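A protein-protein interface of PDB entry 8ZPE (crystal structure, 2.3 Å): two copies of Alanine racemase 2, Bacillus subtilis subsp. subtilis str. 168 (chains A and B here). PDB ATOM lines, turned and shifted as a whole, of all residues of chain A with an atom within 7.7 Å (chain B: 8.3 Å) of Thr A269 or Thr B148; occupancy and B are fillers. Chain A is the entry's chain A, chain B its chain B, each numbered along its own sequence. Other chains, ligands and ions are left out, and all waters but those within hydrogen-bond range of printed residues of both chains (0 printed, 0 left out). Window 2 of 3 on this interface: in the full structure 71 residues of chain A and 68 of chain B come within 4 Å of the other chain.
The backbone carbonyl oxygen of Thr A269 is in hydrogen-bond range of the guanidinium group of Arg B147, at 2.9 Å.
O of Glu A270 is in hydrogen-bond range of NZ of Lys B191, 3.0 Å away.
The guanidinium group (NH2) of Arg B147 lies within hydrogen-bond range of the backbone carbonyl oxygen (O) of Pro A271, 3.2 Å away.
OG1 of Thr A273 is in hydrogen-bond range of O of Gly B140, at 2.8 Å.
Among the printed residues, no Asp or Glu carboxylate lies within 4 Å of a Lys or Arg side-chain nitrogen of the other chain.
O of Met A267 sits at hydrogen-bond distance from NE of Arg A272 (2.9 Å).
OE2 of Glu A270 is in salt-bridge range of NH1 of Arg A272 (3.4 Å).
OD1 of Asp B138 is in hydrogen-bond range of N of Gly B140.
The side-chain carboxylate of Asp B138 is in salt-bridge range of the guanidinium group of Arg B147 (2.9 Å).
The backbone carbonyl oxygen of Arg B147 lies within hydrogen-bond range of the side-chain amino group of Lys B191, 3.4 Å away.
OG1 of Thr B148 is in hydrogen-bond range of N of Glu B151, at 3.2 Å.
No position is printed for both chains.
Of the 8 pairs that touch across the chains among the printed residues, none has its exchanged pair printed and touching as well.
Among the printed residues, pairs that only touch across the chains: Met A267 with Arg B147 (3.7 Å), Thr A269 with Thr B148 (3.9 Å), Pro A271 with Thr B139 (3.5 Å) and Pro A271 with Gly B140 (3.8 Å).
Of chain B, only Arg B147 (2.9 Å) and Thr B148 (3.9 Å) come within 4 Å of Thr A269.
Printed residues of chain B within 4 Å of Glu A270: Lys B191 (3.0 Å).
Of the printed residues of chain B, Pro A271 touches Thr B139, Gly B140 and Arg B147.
Val B137 touches none of the printed residues of chain A.
Printed residues of chain A within 4 Å of Thr B139: Pro A271 (3.5 Å).
Thr B148 touches just one residue of chain A: Thr A269.
Of the printed residues of chain A, Lys B191 touches Glu A270.
The nearest residue of chain A that does not touch Thr B148 is Arg A268 (6.8 Å).
The nearest printed residue of chain B that does not touch Pro A271 is Lys B191 (4.4 Å).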
ATOM      1  N   THR A 266      31.246  16.321  -4.302  1.00  0.00           N
ATOM      2  CA  THR A 266      31.467  17.667  -3.795  1.00  0.00           C
ATOM      3  C   THR A 266      30.395  18.590  -4.357  1.00  0.00           C
ATOM      4  O   THR A 266      29.977  18.449  -5.504  1.00  0.00           O
ATOM      5  CB  THR A 266      32.863  18.168  -4.162  1.00  0.00           C
ATOM      6  OG1 THR A 266      33.840  17.204  -3.755  1.00  0.00           O
ATOM      7  CG2 THR A 266      33.153  19.469  -3.449  1.00  0.00           C
ATOM      8  N   MET A 267      29.938  19.532  -3.538  1.00  0.00           N
ATOM      9  CA  MET A 267      28.795  20.375  -3.897  1.00  0.00           C
ATOM     10  C   MET A 267      29.247  21.689  -4.547  1.00  0.00           C
ATOM     11  O   MET A 267      29.001  22.787  -4.036  1.00  0.00           O
ATOM     12  CB  MET A 267      27.938  20.626  -2.665  1.00  0.00           C
ATOM     13  CG  MET A 267      27.499  19.351  -1.971  1.00  0.00           C
ATOM     14  SD  MET A 267      26.331  18.358  -2.934  1.00  0.00           S
ATOM     15  CE  MET A 267      24.992  19.509  -3.180  1.00  0.00           C
ATOM     16  N   ARG A 268      29.878  21.554  -5.726  1.00  0.00           N
ATOM     17  CA  ARG A 268      30.563  22.671  -6.379  1.00  0.00           C
ATOM     18  C   ARG A 268      29.596  23.620  -7.070  1.00  0.00           C
ATOM     19  O   ARG A 268      29.734  24.842  -6.962  1.00  0.00           O
ATOM     20  CB  ARG A 268      31.581  22.156  -7.396  1.00  0.00           C
ATOM     21  CG  ARG A 268      32.870  21.655  -6.775  1.00  0.00           C
ATOM     22  CD  ARG A 268      33.928  21.320  -7.831  1.00  0.00           C
ATOM     23  NE  ARG A 268      34.954  20.425  -7.304  1.00  0.00           N
ATOM     24  CZ  ARG A 268      35.857  20.762  -6.391  1.00  0.00           C
ATOM     25  NH1 ARG A 268      35.924  21.992  -5.903  1.00  0.00           N
ATOM     26  NH2 ARG A 268      36.712  19.841  -5.951  1.00  0.00           N
ATOM     27  N   THR A 269      28.633  23.091  -7.803  1.00  0.00           N
ATOM     28  CA  THR A 269      27.763  23.929  -8.612  1.00  0.00           C
ATOM     29  C   THR A 269      26.451  24.207  -7.883  1.00  0.00           C
ATOM     30  O   THR A 269      26.073  23.509  -6.941  1.00  0.00           O
ATOM     31  CB  THR A 269      27.494  23.276  -9.978  1.00  0.00           C
ATOM     32  OG1 THR A 269      27.386  21.849  -9.833  1.00  0.00           O
ATOM     33  CG2 THR A 269      28.638  23.587 -10.943  1.00  0.00           C
ATOM     34  N   GLU A 270      25.782  25.215  -8.317  1.00  0.00           N
ATOM     35  CA  GLU A 270      24.507  25.538  -7.696  1.00  0.00           C
ATOM     36  C   GLU A 270      23.360  24.858  -8.431  1.00  0.00           C
ATOM     37  O   GLU A 270      23.465  24.573  -9.626  1.00  0.00           O
ATOM     38  CB  GLU A 270      24.282  27.042  -7.693  1.00  0.00           C
ATOM     39  CG  GLU A 270      24.819  27.702  -6.456  1.00  0.00           C
ATOM     40  CD  GLU A 270      25.321  29.092  -6.729  1.00  0.00           C
ATOM     41  OE1 GLU A 270      24.524  30.045  -6.552  1.00  0.00           O
ATOM     42  OE2 GLU A 270      26.511  29.228  -7.106  1.00  0.00           O
ATOM     43  N   PRO A 271      22.252  24.572  -7.735  1.00  0.00           N
ATOM     44  CA  PRO A 271      22.034  24.789  -6.298  1.00  0.00           C
ATOM     45  C   PRO A 271      22.636  23.703  -5.398  1.00  0.00           C
ATOM     46  O   PRO A 271      22.699  22.540  -5.797  1.00  0.00           O
ATOM     47  CB  PRO A 271      20.508  24.810  -6.187  1.00  0.00           C
ATOM     48  CG  PRO A 271      20.044  23.961  -7.303  1.00  0.00           C
ATOM     49  CD  PRO A 271      21.026  24.143  -8.427  1.00  0.00           C
ATOM     50  N   ARG A 272      23.095  24.097  -4.206  1.00  0.00           N
ATOM     51  CA  ARG A 272      23.685  23.202  -3.214  1.00  0.00           C
ATOM     52  C   ARG A 272      22.659  22.683  -2.215  1.00  0.00           C
ATOM     53  O   ARG A 272      23.023  22.291  -1.100  1.00  0.00           O
ATOM     54  CB  ARG A 272      24.825  23.905  -2.465  1.00  0.00           C
ATOM     55  CG  ARG A 272      25.855  24.509  -3.386  1.00  0.00           C
ATOM     56  CD  ARG A 272      27.010  25.169  -2.660  1.00  0.00           C
ATOM     57  NE  ARG A 272      28.056  25.484  -3.628  1.00  0.00           N
ATOM     58  CZ  ARG A 272      28.054  26.561  -4.400  1.00  0.00           C
ATOM     59  NH1 ARG A 272      27.150  27.515  -4.248  1.00  0.00           N
ATOM     60  NH2 ARG A 272      28.973  26.679  -5.354  1.00  0.00           N
ATOM     61  N   THR A 273      21.395  22.674  -2.603  1.00  0.00           N
ATOM     62  CA  THR A 273      20.312  22.150  -1.792  1.00  0.00           C
ATOM     63  C   THR A 273      20.354  20.625  -1.714  1.00  0.00           C
ATOM     64  O   THR A 273      20.723  19.941  -2.678  1.00  0.00           O
ATOM     65  CB  THR A 273      19.009  22.596  -2.411  1.00  0.00           C
ATOM     66  OG1 THR A 273      19.149  22.469  -3.838  1.00  0.00           O
ATOM     67  CG2 THR A 273      18.767  24.054  -2.057  1.00  0.00           C
ATOM     68  N   ALA A 282      24.571  22.925   1.410  1.00  0.00           N
ATOM     69  CA  ALA A 282      25.936  22.507   1.674  1.00  0.00           C
ATOM     70  C   ALA A 282      26.927  23.584   1.247  1.00  0.00           C
ATOM     71  O   ALA A 282      26.606  24.499   0.485  1.00  0.00           O
ATOM     72  CB  ALA A 282      26.243  21.197   0.940  1.00  0.00           C
ATOM     73  N   GLU A 283      28.150  23.449   1.733  1.00  0.00           N
ATOM     74  CA  GLU A 283      29.194  24.388   1.377  1.00  0.00           C
ATOM     75  C   GLU A 283      29.823  24.019   0.034  1.00  0.00           C
ATOM     76  O   GLU A 283      29.816  22.849  -0.366  1.00  0.00           O
ATOM     77  CB  GLU A 283      30.255  24.411   2.472  1.00  0.00           C
ATOM     78  CG  GLU A 283      29.864  25.178   3.756  1.00  0.00           C
ATOM     79  CD  GLU A 283      29.109  26.503   3.545  1.00  0.00           C
ATOM     80  OE1 GLU A 283      28.974  27.026   2.410  1.00  0.00           O
ATOM     81  OE2 GLU A 283      28.645  27.050   4.564  1.00  0.00           O
ATOM     82  N   PRO A 284      30.413  25.004  -0.665  1.00  0.00           N
ATOM     83  CA  PRO A 284      30.919  24.750  -2.027  1.00  0.00           C
ATOM     84  C   PRO A 284      31.840  23.556  -2.143  1.00  0.00           C
ATOM     85  O   PRO A 284      31.848  22.889  -3.185  1.00  0.00           O
ATOM     86  CB  PRO A 284      31.652  26.052  -2.360  1.00  0.00           C
ATOM     87  CG  PRO A 284      30.941  27.078  -1.577  1.00  0.00           C
ATOM     88  CD  PRO A 284      30.573  26.417  -0.283  1.00  0.00           C
ATOM     89  N   ASN B 136      20.022   9.709 -14.368  1.00  0.00           N
ATOM     90  CA  ASN B 136      19.497  10.579 -13.326  1.00  0.00           C
ATOM     91  C   ASN B 136      20.289  11.876 -13.364  1.00  0.00           C
ATOM     92  O   ASN B 136      21.514  11.873 -13.187  1.00  0.00           O
ATOM     93  CB  ASN B 136      19.613   9.904 -11.952  1.00  0.00           C
ATOM     94  CG  ASN B 136      18.991  10.728 -10.813  1.00  0.00           C
ATOM     95  OD1 ASN B 136      18.679  11.908 -10.963  1.00  0.00           O
ATOM     96  ND2 ASN B 136      18.818  10.091  -9.660  1.00  0.00           N
ATOM     97  N   VAL B 137      19.605  12.983 -13.611  1.00  0.00           N
ATOM     98  CA  VAL B 137      20.254  14.284 -13.578  1.00  0.00           C
ATOM     99  C   VAL B 137      19.847  14.965 -12.280  1.00  0.00           C
ATOM    100  O   VAL B 137      18.653  15.124 -12.006  1.00  0.00           O
ATOM    101  CB  VAL B 137      19.899  15.132 -14.808  1.00  0.00           C
ATOM    102  CG1 VAL B 137      20.524  16.521 -14.684  1.00  0.00           C
ATOM    103  CG2 VAL B 137      20.394  14.447 -16.060  1.00  0.00           C
ATOM    104  N   ASP B 138      20.839  15.330 -11.470  1.00  0.00           N
ATOM    105  CA  ASP B 138      20.619  16.012 -10.200  1.00  0.00           C
ATOM    106  C   ASP B 138      20.618  17.520 -10.447  1.00  0.00           C
ATOM    107  O   ASP B 138      21.678  18.123 -10.640  1.00  0.00           O
ATOM    108  CB  ASP B 138      21.699  15.609  -9.192  1.00  0.00           C
ATOM    109  CG  ASP B 138      21.615  16.393  -7.878  1.00  0.00           C
ATOM    110  OD1 ASP B 138      20.556  17.004  -7.578  1.00  0.00           O
ATOM    111  OD2 ASP B 138      22.621  16.394  -7.144  1.00  0.00           O
ATOM    112  N   THR B 139      19.433  18.129 -10.432  1.00  0.00           N
ATOM    113  CA  THR B 139      19.281  19.563 -10.658  1.00  0.00           C
ATOM    114  C   THR B 139      18.980  20.333  -9.383  1.00  0.00           C
ATOM    115  O   THR B 139      18.743  21.540  -9.446  1.00  0.00           O
ATOM    116  CB  THR B 139      18.187  19.824 -11.687  1.00  0.00           C
ATOM    117  OG1 THR B 139      16.989  19.146 -11.285  1.00  0.00           O
ATOM    118  CG2 THR B 139      18.627  19.326 -13.078  1.00  0.00           C
ATOM    119  N   GLY B 140      18.993  19.669  -8.226  1.00  0.00           N
ATOM    120  CA  GLY B 140      18.857  20.358  -6.965  1.00  0.00           C
ATOM    121  C   GLY B 140      18.380  19.478  -5.829  1.00  0.00           C
ATOM    122  O   GLY B 140      18.206  19.944  -4.704  1.00  0.00           O
ATOM    123  N   GLY B 145      22.797  11.297  -8.910  1.00  0.00           N
ATOM    124  CA  GLY B 145      22.659  11.778 -10.268  1.00  0.00           C
ATOM    125  C   GLY B 145      23.730  12.789 -10.646  1.00  0.00           C
ATOM    126  O   GLY B 145      24.369  13.421  -9.800  1.00  0.00           O
ATOM    127  N   VAL B 146      23.897  12.950 -11.956  1.00  0.00           N
ATOM    128  CA  VAL B 146      24.958  13.782 -12.508  1.00  0.00           C
ATOM    129  C   VAL B 146      24.522  15.239 -12.421  1.00  0.00           C
ATOM    130  O   VAL B 146      23.328  15.560 -12.514  1.00  0.00           O
ATOM    131  CB  VAL B 146      25.287  13.344 -13.959  1.00  0.00           C
ATOM    132  CG1 VAL B 146      24.014  13.217 -14.808  1.00  0.00           C
ATOM    133  CG2 VAL B 146      26.298  14.271 -14.611  1.00  0.00           C
ATOM    134  N   ARG B 147      25.494  16.139 -12.201  1.00  0.00           N
ATOM    135  CA  ARG B 147      25.184  17.499 -11.785  1.00  0.00           C
ATOM    136  C   ARG B 147      25.558  18.597 -12.776  1.00  0.00           C
ATOM    137  O   ARG B 147      25.021  19.702 -12.652  1.00  0.00           O
ATOM    138  CB  ARG B 147      25.849  17.794 -10.430  1.00  0.00           C
ATOM    139  CG  ARG B 147      25.061  17.221  -9.265  1.00  0.00           C
ATOM    140  CD  ARG B 147      25.758  17.411  -7.921  1.00  0.00           C
ATOM    141  NE  ARG B 147      25.906  18.812  -7.559  1.00  0.00           N
ATOM    142  CZ  ARG B 147      24.959  19.532  -6.974  1.00  0.00           C
ATOM    143  NH1 ARG B 147      23.763  19.024  -6.717  1.00  0.00           N
ATOM    144  NH2 ARG B 147      25.212  20.798  -6.651  1.00  0.00           N
ATOM    145  N   THR B 148      26.450  18.349 -13.741  1.00  0.00           N
ATOM    146  CA  THR B 148      26.827  19.367 -14.718  1.00  0.00           C
ATOM    147  C   THR B 148      26.625  18.861 -16.140  1.00  0.00           C
ATOM    148  O   THR B 148      26.577  17.654 -16.387  1.00  0.00           O
ATOM    149  CB  THR B 148      28.284  19.791 -14.566  1.00  0.00           C
ATOM    150  OG1 THR B 148      29.124  18.722 -15.008  1.00  0.00           O
ATOM    151  CG2 THR B 148      28.598  20.115 -13.125  1.00  0.00           C
ATOM    152  N   LYS B 149      26.543  19.804 -17.086  1.00  0.00           N
ATOM    153  CA  LYS B 149      26.288  19.434 -18.477  1.00  0.00           C
ATOM    154  C   LYS B 149      27.472  18.686 -19.069  1.00  0.00           C
ATOM    155  O   LYS B 149      27.289  17.768 -19.873  1.00  0.00           O
ATOM    156  CB  LYS B 149      25.953  20.668 -19.325  1.00  0.00           C
ATOM    157  CG  LYS B 149      27.032  21.752 -19.363  1.00  0.00           C
ATOM    158  CD  LYS B 149      26.594  22.995 -20.170  1.00  0.00           C
ATOM    159  CE  LYS B 149      25.158  23.459 -19.828  1.00  0.00           C
ATOM    160  NZ  LYS B 149      25.068  24.546 -18.777  1.00  0.00           N
ATOM    161  N   GLU B 150      28.691  19.048 -18.675  1.00  0.00           N
ATOM    162  CA  GLU B 150      29.862  18.345 -19.190  1.00  0.00           C
ATOM    163  C   GLU B 150      29.865  16.896 -18.733  1.00  0.00           C
ATOM    164  O   GLU B 150      30.052  15.977 -19.540  1.00  0.00           O
ATOM    165  CB  GLU B 150      31.142  19.055 -18.746  1.00  0.00           C
ATOM    166  CG  GLU B 150      31.274  20.478 -19.255  1.00  0.00           C
ATOM    167  CD  GLU B 150      30.749  21.484 -18.242  1.00  0.00           C
ATOM    168  OE1 GLU B 150      30.922  21.239 -17.021  1.00  0.00           O
ATOM    169  OE2 GLU B 150      30.181  22.520 -18.660  1.00  0.00           O
ATOM    170  N   GLU B 151      29.654  16.673 -17.432  1.00  0.00           N
ATOM    171  CA  GLU B 151      29.636  15.315 -16.900  1.00  0.00           C
ATOM    172  C   GLU B 151      28.521  14.492 -17.530  1.00  0.00           C
ATOM    173  O   GLU B 151      28.733  13.340 -17.917  1.00  0.00           O
ATOM    174  CB  GLU B 151      29.479  15.372 -15.384  1.00  0.00           C
ATOM    175  CG  GLU B 151      29.913  14.138 -14.648  1.00  0.00           C
ATOM    176  CD  GLU B 151      29.854  14.336 -13.147  1.00  0.00           C
ATOM    177  OE1 GLU B 151      28.796  14.789 -12.634  1.00  0.00           O
ATOM    178  OE2 GLU B 151      30.878  14.060 -12.486  1.00  0.00           O
ATOM    179  N   LEU B 152      27.331  15.075 -17.646  1.00  0.00           N
ATOM    180  CA  LEU B 152      26.215  14.398 -18.293  1.00  0.00           C
ATOM    181  C   LEU B 152      26.554  13.992 -19.728  1.00  0.00           C
ATOM    182  O   LEU B 152      26.239  12.873 -20.154  1.00  0.00           O
ATOM    183  CB  LEU B 152      24.987  15.304 -18.260  1.00  0.00           C
ATOM    184  CG  LEU B 152      23.816  15.027 -19.206  1.00  0.00           C
ATOM    185  CD1 LEU B 152      23.211  13.652 -18.964  1.00  0.00           C
ATOM    186  CD2 LEU B 152      22.752  16.112 -19.009  1.00  0.00           C
ATOM    187  N   LEU B 153      27.190  14.892 -20.494  1.00  0.00           N
ATOM    188  CA  LEU B 153      27.587  14.550 -21.859  1.00  0.00           C
ATOM    189  C   LEU B 153      28.523  13.351 -21.874  1.00  0.00           C
ATOM    190  O   LEU B 153      28.369  12.439 -22.700  1.00  0.00           O
ATOM    191  CB  LEU B 153      28.255  15.744 -22.542  1.00  0.00           C
ATOM    192  CG  LEU B 153      28.753  15.486 -23.972  1.00  0.00           C
ATOM    193  CD1 LEU B 153      27.610  14.994 -24.875  1.00  0.00           C
ATOM    194  CD2 LEU B 153      29.414  16.725 -24.560  1.00  0.00           C
ATOM    195  N   GLU B 154      29.501  13.337 -20.963  1.00  0.00           N
ATOM    196  CA  GLU B 154      30.410  12.202 -20.873  1.00  0.00           C
ATOM    197  C   GLU B 154      29.648  10.932 -20.539  1.00  0.00           C
ATOM    198  O   GLU B 154      29.958   9.857 -21.067  1.00  0.00           O
ATOM    199  CB  GLU B 154      31.497  12.470 -19.831  1.00  0.00           C
ATOM    200  CG  GLU B 154      32.768  13.048 -20.432  1.00  0.00           C
ATOM    201  CD  GLU B 154      33.838  13.325 -19.389  1.00  0.00           C
ATOM    202  OE1 GLU B 154      33.644  12.927 -18.220  1.00  0.00           O
ATOM    203  OE2 GLU B 154      34.874  13.935 -19.742  1.00  0.00           O
ATOM    204  N   VAL B 155      28.625  11.046 -19.683  1.00  0.00           N
ATOM    205  CA  VAL B 155      27.843   9.878 -19.293  1.00  0.00           C
ATOM    206  C   VAL B 155      27.002   9.387 -20.463  1.00  0.00           C
ATOM    207  O   VAL B 155      26.930   8.180 -20.733  1.00  0.00           O
ATOM    208  CB  VAL B 155      26.977  10.203 -18.062  1.00  0.00           C
ATOM    209  CG1 VAL B 155      26.009   9.056 -17.775  1.00  0.00           C
ATOM    210  CG2 VAL B 155      27.862  10.502 -16.854  1.00  0.00           C
ATOM    211  N   LYS B 191      17.334  24.304 -15.497  1.00  0.00           N
ATOM    212  CA  LYS B 191      18.577  23.559 -15.630  1.00  0.00           C
ATOM    213  C   LYS B 191      18.354  22.288 -16.440  1.00  0.00           C
ATOM    214  O   LYS B 191      19.075  22.022 -17.405  1.00  0.00           O
ATOM    215  CB  LYS B 191      19.136  23.234 -14.248  1.00  0.00           C
ATOM    216  CG  LYS B 191      20.647  23.293 -14.176  1.00  0.00           C
ATOM    217  CD  LYS B 191      21.140  23.216 -12.740  1.00  0.00           C
ATOM    218  CE  LYS B 191      22.553  23.714 -12.630  1.00  0.00           C
ATOM    219  NZ  LYS B 191      23.433  22.689 -11.998  1.00  0.00           N
ATOM    220  N   PHE B 195      20.046  21.317 -20.106  1.00  0.00           N
ATOM    221  CA  PHE B 195      20.923  20.164 -20.300  1.00  0.00           C
ATOM    222  C   PHE B 195      20.451  19.298 -21.462  1.00  0.00           C
ATOM    223  O   PHE B 195      21.257  18.870 -22.293  1.00  0.00           O
ATOM    224  CB  PHE B 195      20.997  19.333 -19.021  1.00  0.00           C
ATOM    225  CG  PHE B 195      21.808  19.962 -17.923  1.00  0.00           C
ATOM    226  CD1 PHE B 195      22.123  21.309 -17.948  1.00  0.00           C
ATOM    227  CD2 PHE B 195      22.257  19.193 -16.860  1.00  0.00           C
ATOM    228  CE1 PHE B 195      22.868  21.876 -16.923  1.00  0.00           C
ATOM    229  CE2 PHE B 195      22.997  19.747 -15.838  1.00  0.00           C
ATOM    230  CZ  PHE B 195      23.311  21.088 -15.866  1.00  0.00           C
ATOM    231  N   PHE B 198      21.160  21.291 -24.431  1.00  0.00           N
ATOM    232  CA  PHE B 198      22.591  21.157 -24.674  1.00  0.00           C
ATOM    233  C   PHE B 198      22.889  19.848 -25.384  1.00  0.00           C
ATOM    234  O   PHE B 198      23.716  19.801 -26.296  1.00  0.00           O
ATOM    235  CB  PHE B 198      23.366  21.245 -23.361  1.00  0.00           C
ATOM    236  CG  PHE B 198      24.826  20.855 -23.473  1.00  0.00           C
ATOM    237  CD1 PHE B 198      25.234  19.541 -23.302  1.00  0.00           C
ATOM    238  CD2 PHE B 198      25.793  21.810 -23.719  1.00  0.00           C
ATOM    239  CE1 PHE B 198      26.578  19.193 -23.381  1.00  0.00           C
ATOM    240  CE2 PHE B 198      27.140  21.467 -23.800  1.00  0.00           C
ATOM    241  CZ  PHE B 198      27.529  20.161 -23.632  1.00  0.00           C
ATOM    242  N   LEU B 199      22.220  18.773 -24.977  1.00  0.00           N
ATOM    243  CA  LEU B 199      22.457  17.487 -25.613  1.00  0.00           C
ATOM    244  C   LEU B 199      21.945  17.484 -27.043  1.00  0.00           C
ATOM    245  O   LEU B 199      22.632  16.997 -27.946  1.00  0.00           O
ATOM    246  CB  LEU B 199      21.797  16.367 -24.805  1.00  0.00           C
ATOM    247  CG  LEU B 199      22.440  15.961 -23.477  1.00  0.00           C
ATOM    248  CD1 LEU B 199      21.701  14.772 -22.912  1.00  0.00           C
ATOM    249  CD2 LEU B 199      23.914  15.642 -23.638  1.00  0.00           C
